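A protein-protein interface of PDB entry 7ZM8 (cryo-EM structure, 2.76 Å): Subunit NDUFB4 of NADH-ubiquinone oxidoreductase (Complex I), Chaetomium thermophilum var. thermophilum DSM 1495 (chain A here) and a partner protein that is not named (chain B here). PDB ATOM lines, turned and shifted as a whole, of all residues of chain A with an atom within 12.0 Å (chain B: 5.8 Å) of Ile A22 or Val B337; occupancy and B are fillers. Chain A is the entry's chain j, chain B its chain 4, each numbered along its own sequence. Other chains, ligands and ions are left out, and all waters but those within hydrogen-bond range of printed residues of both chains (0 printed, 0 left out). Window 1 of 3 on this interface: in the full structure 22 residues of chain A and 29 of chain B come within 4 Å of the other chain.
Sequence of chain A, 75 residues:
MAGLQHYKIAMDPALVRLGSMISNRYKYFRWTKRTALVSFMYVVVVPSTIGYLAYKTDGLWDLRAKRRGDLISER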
ATOM      1  N   MET A  11      -8.466 -10.307   4.837  1.00  0.00           N
ATOM      2  CA  MET A  11      -8.731 -11.558   4.099  1.00  0.00           C
ATOM      3  C   MET A  11      -7.468 -11.941   3.364  1.00  0.00           C
ATOM      4  O   MET A  11      -6.990 -11.151   2.543  1.00  0.00           O
ATOM      5  CB  MET A  11      -9.849 -11.327   3.095  1.00  0.00           C
ATOM      6  CG  MET A  11     -11.215 -11.501   3.718  1.00  0.00           C
ATOM      7  SD  MET A  11     -11.453 -13.222   4.210  1.00  0.00           S
ATOM      8  CE  MET A  11     -12.432 -13.017   5.693  1.00  0.00           C
ATOM      9  N   PRO A  13      -5.443 -13.364   0.581  1.00  0.00           N
ATOM     10  CA  PRO A  13      -5.688 -13.890  -0.769  1.00  0.00           C
ATOM     11  C   PRO A  13      -5.357 -15.361  -0.905  1.00  0.00           C
ATOM     12  O   PRO A  13      -6.000 -16.061  -1.694  1.00  0.00           O
ATOM     13  CB  PRO A  13      -4.780 -13.021  -1.647  1.00  0.00           C
ATOM     14  CG  PRO A  13      -4.556 -11.791  -0.864  1.00  0.00           C
ATOM     15  CD  PRO A  13      -4.542 -12.202   0.566  1.00  0.00           C
ATOM     16  N   ALA A  14      -4.368 -15.852  -0.157  1.00  0.00           N
ATOM     17  CA  ALA A  14      -3.974 -17.250  -0.265  1.00  0.00           C
ATOM     18  C   ALA A  14      -5.010 -18.172   0.359  1.00  0.00           C
ATOM     19  O   ALA A  14      -5.303 -19.240  -0.183  1.00  0.00           O
ATOM     20  CB  ALA A  14      -2.611 -17.456   0.392  1.00  0.00           C
ATOM     21  N   LEU A  15      -5.558 -17.789   1.511  1.00  0.00           N
ATOM     22  CA  LEU A  15      -6.581 -18.611   2.145  1.00  0.00           C
ATOM     23  C   LEU A  15      -7.919 -18.488   1.432  1.00  0.00           C
ATOM     24  O   LEU A  15      -8.707 -19.438   1.433  1.00  0.00           O
ATOM     25  CB  LEU A  15      -6.720 -18.227   3.614  1.00  0.00           C
ATOM     26  CG  LEU A  15      -5.429 -18.270   4.424  1.00  0.00           C
ATOM     27  CD1 LEU A  15      -5.645 -17.636   5.776  1.00  0.00           C
ATOM     28  CD2 LEU A  15      -4.958 -19.695   4.578  1.00  0.00           C
ATOM     29  N   VAL A  16      -8.199 -17.330   0.834  1.00  0.00           N
ATOM     30  CA  VAL A  16      -9.444 -17.163   0.090  1.00  0.00           C
ATOM     31  C   VAL A  16      -9.455 -18.050  -1.147  1.00  0.00           C
ATOM     32  O   VAL A  16     -10.464 -18.693  -1.457  1.00  0.00           O
ATOM     33  CB  VAL A  16      -9.656 -15.680  -0.262  1.00  0.00           C
ATOM     34  CG1 VAL A  16     -10.662 -15.530  -1.378  1.00  0.00           C
ATOM     35  CG2 VAL A  16     -10.123 -14.918   0.959  1.00  0.00           C
ATOM     36  N   ARG A  17      -8.338 -18.107  -1.872  1.00  0.00           N
ATOM     37  CA  ARG A  17      -8.284 -18.964  -3.048  1.00  0.00           C
ATOM     38  C   ARG A  17      -8.236 -20.438  -2.669  1.00  0.00           C
ATOM     39  O   ARG A  17      -8.681 -21.286  -3.445  1.00  0.00           O
ATOM     40  CB  ARG A  17      -7.090 -18.586  -3.924  1.00  0.00           C
ATOM     41  CG  ARG A  17      -5.740 -18.880  -3.330  1.00  0.00           C
ATOM     42  CD  ARG A  17      -4.663 -18.828  -4.389  1.00  0.00           C
ATOM     43  NE  ARG A  17      -3.394 -18.338  -3.861  1.00  0.00           N
ATOM     44  CZ  ARG A  17      -3.022 -17.063  -3.869  1.00  0.00           C
ATOM     45  NH1 ARG A  17      -1.850 -16.710  -3.363  1.00  0.00           N
ATOM     46  NH2 ARG A  17      -3.823 -16.137  -4.380  1.00  0.00           N
ATOM     47  N   LEU A  18      -7.703 -20.761  -1.487  1.00  0.00           N
ATOM     48  CA  LEU A  18      -7.756 -22.134  -0.997  1.00  0.00           C
ATOM     49  C   LEU A  18      -9.183 -22.556  -0.678  1.00  0.00           C
ATOM     50  O   LEU A  18      -9.603 -23.660  -1.035  1.00  0.00           O
ATOM     51  CB  LEU A  18      -6.877 -22.286   0.240  1.00  0.00           C
ATOM     52  CG  LEU A  18      -6.971 -23.635   0.954  1.00  0.00           C
ATOM     53  CD1 LEU A  18      -6.475 -24.753   0.076  1.00  0.00           C
ATOM     54  CD2 LEU A  18      -6.229 -23.604   2.266  1.00  0.00           C
ATOM     55  N   GLY A  19      -9.933 -21.701   0.012  1.00  0.00           N
ATOM     56  CA  GLY A  19     -11.323 -22.013   0.286  1.00  0.00           C
ATOM     57  C   GLY A  19     -12.156 -22.092  -0.972  1.00  0.00           C
ATOM     58  O   GLY A  19     -13.098 -22.882  -1.050  1.00  0.00           O
ATOM     59  N   SER A  20     -11.830 -21.268  -1.968  1.00  0.00           N
ATOM     60  CA  SER A  20     -12.463 -21.399  -3.273  1.00  0.00           C
ATOM     61  C   SER A  20     -12.102 -22.726  -3.925  1.00  0.00           C
ATOM     62  O   SER A  20     -12.947 -23.358  -4.565  1.00  0.00           O
ATOM     63  CB  SER A  20     -12.058 -20.230  -4.166  1.00  0.00           C
ATOM     64  OG  SER A  20     -12.538 -19.009  -3.639  1.00  0.00           O
ATOM     65  N   MET A  21     -10.849 -23.157  -3.779  1.00  0.00           N
ATOM     66  CA  MET A  21     -10.432 -24.427  -4.361  1.00  0.00           C
ATOM     67  C   MET A  21     -11.212 -25.586  -3.759  1.00  0.00           C
ATOM     68  O   MET A  21     -11.644 -26.492  -4.478  1.00  0.00           O
ATOM     69  CB  MET A  21      -8.930 -24.623  -4.161  1.00  0.00           C
ATOM     70  CG  MET A  21      -8.332 -25.814  -4.899  1.00  0.00           C
ATOM     71  SD  MET A  21      -8.481 -27.388  -4.025  1.00  0.00           S
ATOM     72  CE  MET A  21      -7.283 -27.167  -2.722  1.00  0.00           C
ATOM     73  N   ILE A  22     -11.374 -25.598  -2.444  1.00  0.00           N
ATOM     74  CA  ILE A  22     -12.068 -26.734  -1.776  1.00  0.00           C
ATOM     75  C   ILE A  22     -13.516 -26.782  -2.286  1.00  0.00           C
ATOM     76  O   ILE A  22     -13.992 -27.880  -2.603  1.00  0.00           O
ATOM     77  CB  ILE A  22     -11.915 -26.583  -0.250  1.00  0.00           C
ATOM     78  CG1 ILE A  22     -10.473 -26.866   0.170  1.00  0.00           C
ATOM     79  CG2 ILE A  22     -12.896 -27.470   0.492  1.00  0.00           C
ATOM     80  CD1 ILE A  22     -10.169 -26.555   1.614  1.00  0.00           C
ATOM     81  N   SER A  23     -14.162 -25.629  -2.442  1.00  0.00           N
ATOM     82  CA  SER A  23     -15.575 -25.541  -2.891  1.00  0.00           C
ATOM     83  C   SER A  23     -15.799 -26.039  -4.320  1.00  0.00           C
ATOM     84  O   SER A  23     -16.841 -26.670  -4.545  1.00  0.00           O
ATOM     85  CB  SER A  23     -16.082 -24.141  -2.747  1.00  0.00           C
ATOM     86  OG  SER A  23     -16.057 -23.741  -1.386  1.00  0.00           O
ATOM     87  N   ASN A  24     -14.890 -25.789  -5.250  1.00  0.00           N
ATOM     88  CA  ASN A  24     -15.153 -26.150  -6.662  1.00  0.00           C
ATOM     89  C   ASN A  24     -14.453 -27.455  -7.017  1.00  0.00           C
ATOM     90  O   ASN A  24     -14.654 -27.918  -8.129  1.00  0.00           O
ATOM     91  CB  ASN A  24     -14.711 -25.000  -7.560  1.00  0.00           C
ATOM     92  CG  ASN A  24     -15.532 -23.747  -7.359  1.00  0.00           C
ATOM     93  OD1 ASN A  24     -16.696 -23.699  -7.742  1.00  0.00           O
ATOM     94  ND2 ASN A  24     -14.933 -22.725  -6.773  1.00  0.00           N
ATOM     95  N   ARG A  25     -13.724 -28.070  -6.089  1.00  0.00           N
ATOM     96  CA  ARG A  25     -12.888 -29.287  -6.322  1.00  0.00           C
ATOM     97  C   ARG A  25     -13.590 -30.419  -7.084  1.00  0.00           C
ATOM     98  O   ARG A  25     -12.908 -31.072  -7.880  1.00  0.00           O
ATOM     99  CB  ARG A  25     -12.361 -29.752  -4.960  1.00  0.00           C
ATOM    100  CG  ARG A  25     -11.336 -30.870  -5.031  1.00  0.00           C
ATOM    101  CD  ARG A  25     -11.018 -31.487  -3.686  1.00  0.00           C
ATOM    102  NE  ARG A  25     -10.206 -32.667  -3.921  1.00  0.00           N
ATOM    103  CZ  ARG A  25      -8.882 -32.689  -3.915  1.00  0.00           C
ATOM    104  NH1 ARG A  25      -8.243 -33.819  -4.155  1.00  0.00           N
ATOM    105  NH2 ARG A  25      -8.200 -31.591  -3.645  1.00  0.00           N
ATOM    106  N   TYR A  26     -14.871 -30.660  -6.832  1.00  0.00           N
ATOM    107  CA  TYR A  26     -15.608 -31.792  -7.451  1.00  0.00           C
ATOM    108  C   TYR A  26     -15.603 -31.660  -8.976  1.00  0.00           C
ATOM    109  O   TYR A  26     -15.575 -32.673  -9.669  1.00  0.00           O
ATOM    110  CB  TYR A  26     -17.031 -31.848  -6.878  1.00  0.00           C
ATOM    111  CG  TYR A  26     -17.925 -30.709  -7.297  1.00  0.00           C
ATOM    112  CD1 TYR A  26     -17.836 -29.471  -6.686  1.00  0.00           C
ATOM    113  CD2 TYR A  26     -18.847 -30.863  -8.319  1.00  0.00           C
ATOM    114  CE1 TYR A  26     -18.638 -28.414  -7.074  1.00  0.00           C
ATOM    115  CE2 TYR A  26     -19.657 -29.816  -8.720  1.00  0.00           C
ATOM    116  CZ  TYR A  26     -19.550 -28.585  -8.098  1.00  0.00           C
ATOM    117  OH  TYR A  26     -20.344 -27.546  -8.484  1.00  0.00           O
ATOM    118  N   LYS A  27     -15.685 -30.443  -9.478  1.00  0.00           N
ATOM    119  CA  LYS A  27     -15.676 -30.194 -10.928  1.00  0.00           C
ATOM    120  C   LYS A  27     -14.418 -30.802 -11.552  1.00  0.00           C
ATOM    121  O   LYS A  27     -14.372 -30.864 -12.790  1.00  0.00           O
ATOM    122  CB  LYS A  27     -15.739 -28.685 -11.138  1.00  0.00           C
ATOM    123  CG  LYS A  27     -17.082 -28.031 -10.865  1.00  0.00           C
ATOM    124  CD  LYS A  27     -16.962 -26.553 -10.600  1.00  0.00           C
ATOM    125  CE  LYS A  27     -15.936 -25.880 -11.483  1.00  0.00           C
ATOM    126  NZ  LYS A  27     -15.823 -24.433 -11.185  1.00  0.00           N
ATOM    127  N   TYR A  28     -13.447 -31.263 -10.746  1.00  0.00           N
ATOM    128  CA  TYR A  28     -12.265 -31.793 -11.409  1.00  0.00           C
ATOM    129  C   TYR A  28     -11.966 -33.240 -11.048  1.00  0.00           C
ATOM    130  O   TYR A  28     -10.884 -33.731 -11.374  1.00  0.00           O
ATOM    131  CB  TYR A  28     -11.043 -30.923 -11.115  1.00  0.00           C
ATOM    132  CG  TYR A  28     -11.270 -29.446 -11.314  1.00  0.00           C
ATOM    133  CD1 TYR A  28     -11.951 -28.688 -10.375  1.00  0.00           C
ATOM    134  CD2 TYR A  28     -10.853 -28.820 -12.476  1.00  0.00           C
ATOM    135  CE1 TYR A  28     -12.168 -27.353 -10.566  1.00  0.00           C
ATOM    136  CE2 TYR A  28     -11.070 -27.486 -12.676  1.00  0.00           C
ATOM    137  CZ  TYR A  28     -11.727 -26.757 -11.721  1.00  0.00           C
ATOM    138  OH  TYR A  28     -11.943 -25.416 -11.927  1.00  0.00           O
ATOM    139  N   PHE A  29     -12.891 -33.942 -10.409  1.00  0.00           N
ATOM    140  CA  PHE A  29     -12.671 -35.350 -10.113  1.00  0.00           C
ATOM    141  C   PHE A  29     -12.737 -36.178 -11.390  1.00  0.00           C
ATOM    142  O   PHE A  29     -13.641 -36.016 -12.212  1.00  0.00           O
ATOM    143  CB  PHE A  29     -13.702 -35.852  -9.101  1.00  0.00           C
ATOM    144  CG  PHE A  29     -13.587 -37.319  -8.790  1.00  0.00           C
ATOM    145  CD1 PHE A  29     -12.737 -37.768  -7.805  1.00  0.00           C
ATOM    146  CD2 PHE A  29     -14.339 -38.243  -9.481  1.00  0.00           C
ATOM    147  CE1 PHE A  29     -12.629 -39.097  -7.523  1.00  0.00           C
ATOM    148  CE2 PHE A  29     -14.231 -39.579  -9.206  1.00  0.00           C
ATOM    149  CZ  PHE A  29     -13.378 -40.007  -8.221  1.00  0.00           C
ATOM    150  N   ARG B 335     -11.933 -33.013   9.122  1.00  0.00           N
ATOM    151  CA  ARG B 335     -11.138 -32.301   8.133  1.00  0.00           C
ATOM    152  C   ARG B 335     -11.925 -31.233   7.386  1.00  0.00           C
ATOM    153  O   ARG B 335     -11.463 -30.745   6.353  1.00  0.00           O
ATOM    154  CB  ARG B 335     -10.532 -33.296   7.146  1.00  0.00           C
ATOM    155  CG  ARG B 335      -9.519 -34.230   7.767  1.00  0.00           C
ATOM    156  CD  ARG B 335      -8.225 -33.529   8.109  1.00  0.00           C
ATOM    157  NE  ARG B 335      -7.606 -32.895   6.954  1.00  0.00           N
ATOM    158  CZ  ARG B 335      -6.788 -33.516   6.113  1.00  0.00           C
ATOM    159  NH1 ARG B 335      -6.497 -34.793   6.292  1.00  0.00           N
ATOM    160  NH2 ARG B 335      -6.269 -32.859   5.087  1.00  0.00           N
ATOM    161  N   THR B 336     -13.091 -30.851   7.889  1.00  0.00           N
ATOM    162  CA  THR B 336     -13.899 -29.823   7.249  1.00  0.00           C
ATOM    163  C   THR B 336     -13.399 -28.442   7.658  1.00  0.00           C
ATOM    164  O   THR B 336     -13.162 -28.182   8.841  1.00  0.00           O
ATOM    165  CB  THR B 336     -15.370 -30.006   7.625  1.00  0.00           C
ATOM    166  OG1 THR B 336     -15.838 -31.250   7.098  1.00  0.00           O
ATOM    167  CG2 THR B 336     -16.220 -28.887   7.059  1.00  0.00           C
ATOM    168  N   VAL B 337     -13.252 -27.540   6.688  1.00  0.00           N
ATOM    169  CA  VAL B 337     -12.664 -26.199   6.970  1.00  0.00           C
ATOM    170  C   VAL B 337     -13.728 -25.094   6.994  1.00  0.00           C
ATOM    171  O   VAL B 337     -13.353 -23.960   7.292  1.00  0.00           O
ATOM    172  CB  VAL B 337     -11.576 -25.898   5.926  1.00  0.00           C
ATOM    173  CG1 VAL B 337     -10.673 -27.098   5.709  1.00  0.00           C
ATOM    174  CG2 VAL B 337     -12.170 -25.451   4.599  1.00  0.00           C
ATOM    175  N   ASP B 338     -14.995 -25.407   6.737  1.00  0.00           N
ATOM    176  CA  ASP B 338     -16.100 -24.418   6.835  1.00  0.00           C
ATOM    177  C   ASP B 338     -16.791 -24.689   8.170  1.00  0.00           C
ATOM    178  O   ASP B 338     -17.142 -25.845   8.397  1.00  0.00           O
ATOM    179  CB  ASP B 338     -17.039 -24.595   5.641  1.00  0.00           C
ATOM    180  CG  ASP B 338     -18.162 -23.581   5.503  1.00  0.00           C
ATOM    181  OD1 ASP B 338     -18.909 -23.381   6.476  1.00  0.00           O
ATOM    182  OD2 ASP B 338     -18.299 -23.022   4.402  1.00  0.00           O
ATOM    183  N   VAL B 339     -16.934 -23.696   9.039  1.00  0.00           N
ATOM    184  CA  VAL B 339     -17.482 -24.008  10.386  1.00  0.00           C
ATOM    185  C   VAL B 339     -18.940 -24.430  10.253  1.00  0.00           C
ATOM    186  O   VAL B 339     -19.337 -25.367  10.943  1.00  0.00           O
ATOM    187  CB  VAL B 339     -17.316 -22.810  11.339  1.00  0.00           C
ATOM    188  CG1 VAL B 339     -17.782 -23.134  12.747  1.00  0.00           C
ATOM    189  CG2 VAL B 339     -15.875 -22.328  11.359  1.00  0.00           C
ATOM    190  N   ARG B 398     -16.740 -18.108   6.797  1.00  0.00           N
ATOM    191  CA  ARG B 398     -16.988 -19.355   7.567  1.00  0.00           C
ATOM    192  C   ARG B 398     -15.734 -20.213   7.639  1.00  0.00           C
ATOM    193  O   ARG B 398     -15.839 -21.327   8.122  1.00  0.00           O
ATOM    194  CB  ARG B 398     -18.183 -20.137   7.024  1.00  0.00           C
ATOM    195  CG  ARG B 398     -19.431 -19.288   6.848  1.00  0.00           C
ATOM    196  CD  ARG B 398     -20.565 -19.805   7.703  1.00  0.00           C
ATOM    197  NE  ARG B 398     -21.824 -19.114   7.479  1.00  0.00           N
ATOM    198  CZ  ARG B 398     -22.627 -19.332   6.448  1.00  0.00           C
ATOM    199  NH1 ARG B 398     -22.299 -20.220   5.527  1.00  0.00           N
ATOM    200  NH2 ARG B 398     -23.755 -18.657   6.337  1.00  0.00           N
ATOM    201  N   LEU B 399     -14.586 -19.694   7.222  1.00  0.00           N
ATOM    202  CA  LEU B 399     -13.374 -20.547   7.173  1.00  0.00           C
ATOM    203  C   LEU B 399     -12.656 -20.584   8.516  1.00  0.00           C
ATOM    204  O   LEU B 399     -12.266 -19.518   8.982  1.00  0.00           O
ATOM    205  CB  LEU B 399     -12.474 -20.122   6.013  1.00  0.00           C
ATOM    206  CG  LEU B 399     -13.061 -20.322   4.621  1.00  0.00           C
ATOM    207  CD1 LEU B 399     -12.051 -19.941   3.555  1.00  0.00           C
ATOM    208  CD2 LEU B 399     -13.523 -21.757   4.428  1.00  0.00           C
ATOM    209  N   ILE B 400     -12.442 -21.780   9.071  1.00  0.00           N
ATOM    210  CA  ILE B 400     -11.828 -21.945  10.380  1.00  0.00           C
ATOM    211  C   ILE B 400     -10.381 -21.478  10.394  1.00  0.00           C
ATOM    212  O   ILE B 400      -9.777 -21.379  11.467  1.00  0.00           O
ATOM    213  CB  ILE B 400     -11.955 -23.418  10.819  1.00  0.00           C
ATOM    214  CG1 ILE B 400     -11.990 -23.524  12.340  1.00  0.00           C
ATOM    215  CG2 ILE B 400     -10.828 -24.257  10.241  1.00  0.00           C
ATOM    216  CD1 ILE B 400     -12.348 -24.889  12.845  1.00  0.00           C
ATOM    217  N   TYR B 401      -9.813 -21.184   9.222  1.00  0.00           N
ATOM    218  CA  TYR B 401      -8.468 -20.630   9.151  1.00  0.00           C
ATOM    219  C   TYR B 401      -8.380 -19.271   9.823  1.00  0.00           C
ATOM    220  O   TYR B 401      -7.343 -18.930  10.399  1.00  0.00           O
ATOM    221  CB  TYR B 401      -8.036 -20.504   7.695  1.00  0.00           C
ATOM    222  CG  TYR B 401      -7.997 -21.808   6.955  1.00  0.00           C
ATOM    223  CD1 TYR B 401      -7.420 -22.926   7.518  1.00  0.00           C
ATOM    224  CD2 TYR B 401      -8.530 -21.916   5.683  1.00  0.00           C
ATOM    225  CE1 TYR B 401      -7.382 -24.113   6.843  1.00  0.00           C
ATOM    226  CE2 TYR B 401      -8.498 -23.104   5.002  1.00  0.00           C
ATOM    227  CZ  TYR B 401      -7.921 -24.197   5.585  1.00  0.00           C
ATOM    228  OH  TYR B 401      -7.881 -25.388   4.907  1.00  0.00           O
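The backbone carbonyl oxygen (O) of Gly A19 lies within hydrogen-bond range of the side-chain hydroxyl (OG) of Ser A23 (3.1 Å).
N of Ile B400 sits at hydrogen-bond distance from O of Val B337.
Among the printed residues, merely in contact across the chains: Leu A15 with Leu B399 (3.99 Å), Leu A18 with Tyr B401 (3.6 Å), Gly A19 with Leu B399 (3.9 Å) and Ile A22 with Val B337 (3.8 Å).
Of the printed residues of chain B, Leu A15 touches Leu B399 (3.99 Å).
Of the printed residues of chain B, Leu A18 touches Tyr B401 (3.6 Å).
Of the printed residues of chain B, Gly A19 touches Leu B399 (3.9 Å).
Lys A27 touches none of the printed residues of chain B.
No residue of chain A comes within 4 Å of Thr B336.
Val B337 touches just one residue of chain A: Ile A22 (3.8 Å).
No residue of chain A comes within 4 Å of Asp B338.
Val B339 touches none of the printed residues of chain A.
Printed residues of chain A within 4 Å of Leu B399: Leu A15 (3.99 Å) and Gly A19 (3.9 Å).
No residue of chain A comes within 4 Å of Ile B400.
Of the printed residues of chain A, Tyr B401 touches Leu A18 (3.6 Å).
The nearest residue of chain A that does not touch Val B337 is Gly A19 (5.6 Å).
Of the 18 printed residues of chain A, 4 touch a printed residue of chain B.
Printed residues of chain A that touch a printed residue of chain B: Leu A15, Leu A18, Gly A19 and Ile A22.
Hydrophobic or aromatic side chains of chain A within 4 Å of the printed part of chain B: Leu A18 and Ile A22.
Among the printed residues, no Asp or Glu carboxylate lies within 4 Å of a Lys or Arg side-chain nitrogen of the other chain.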
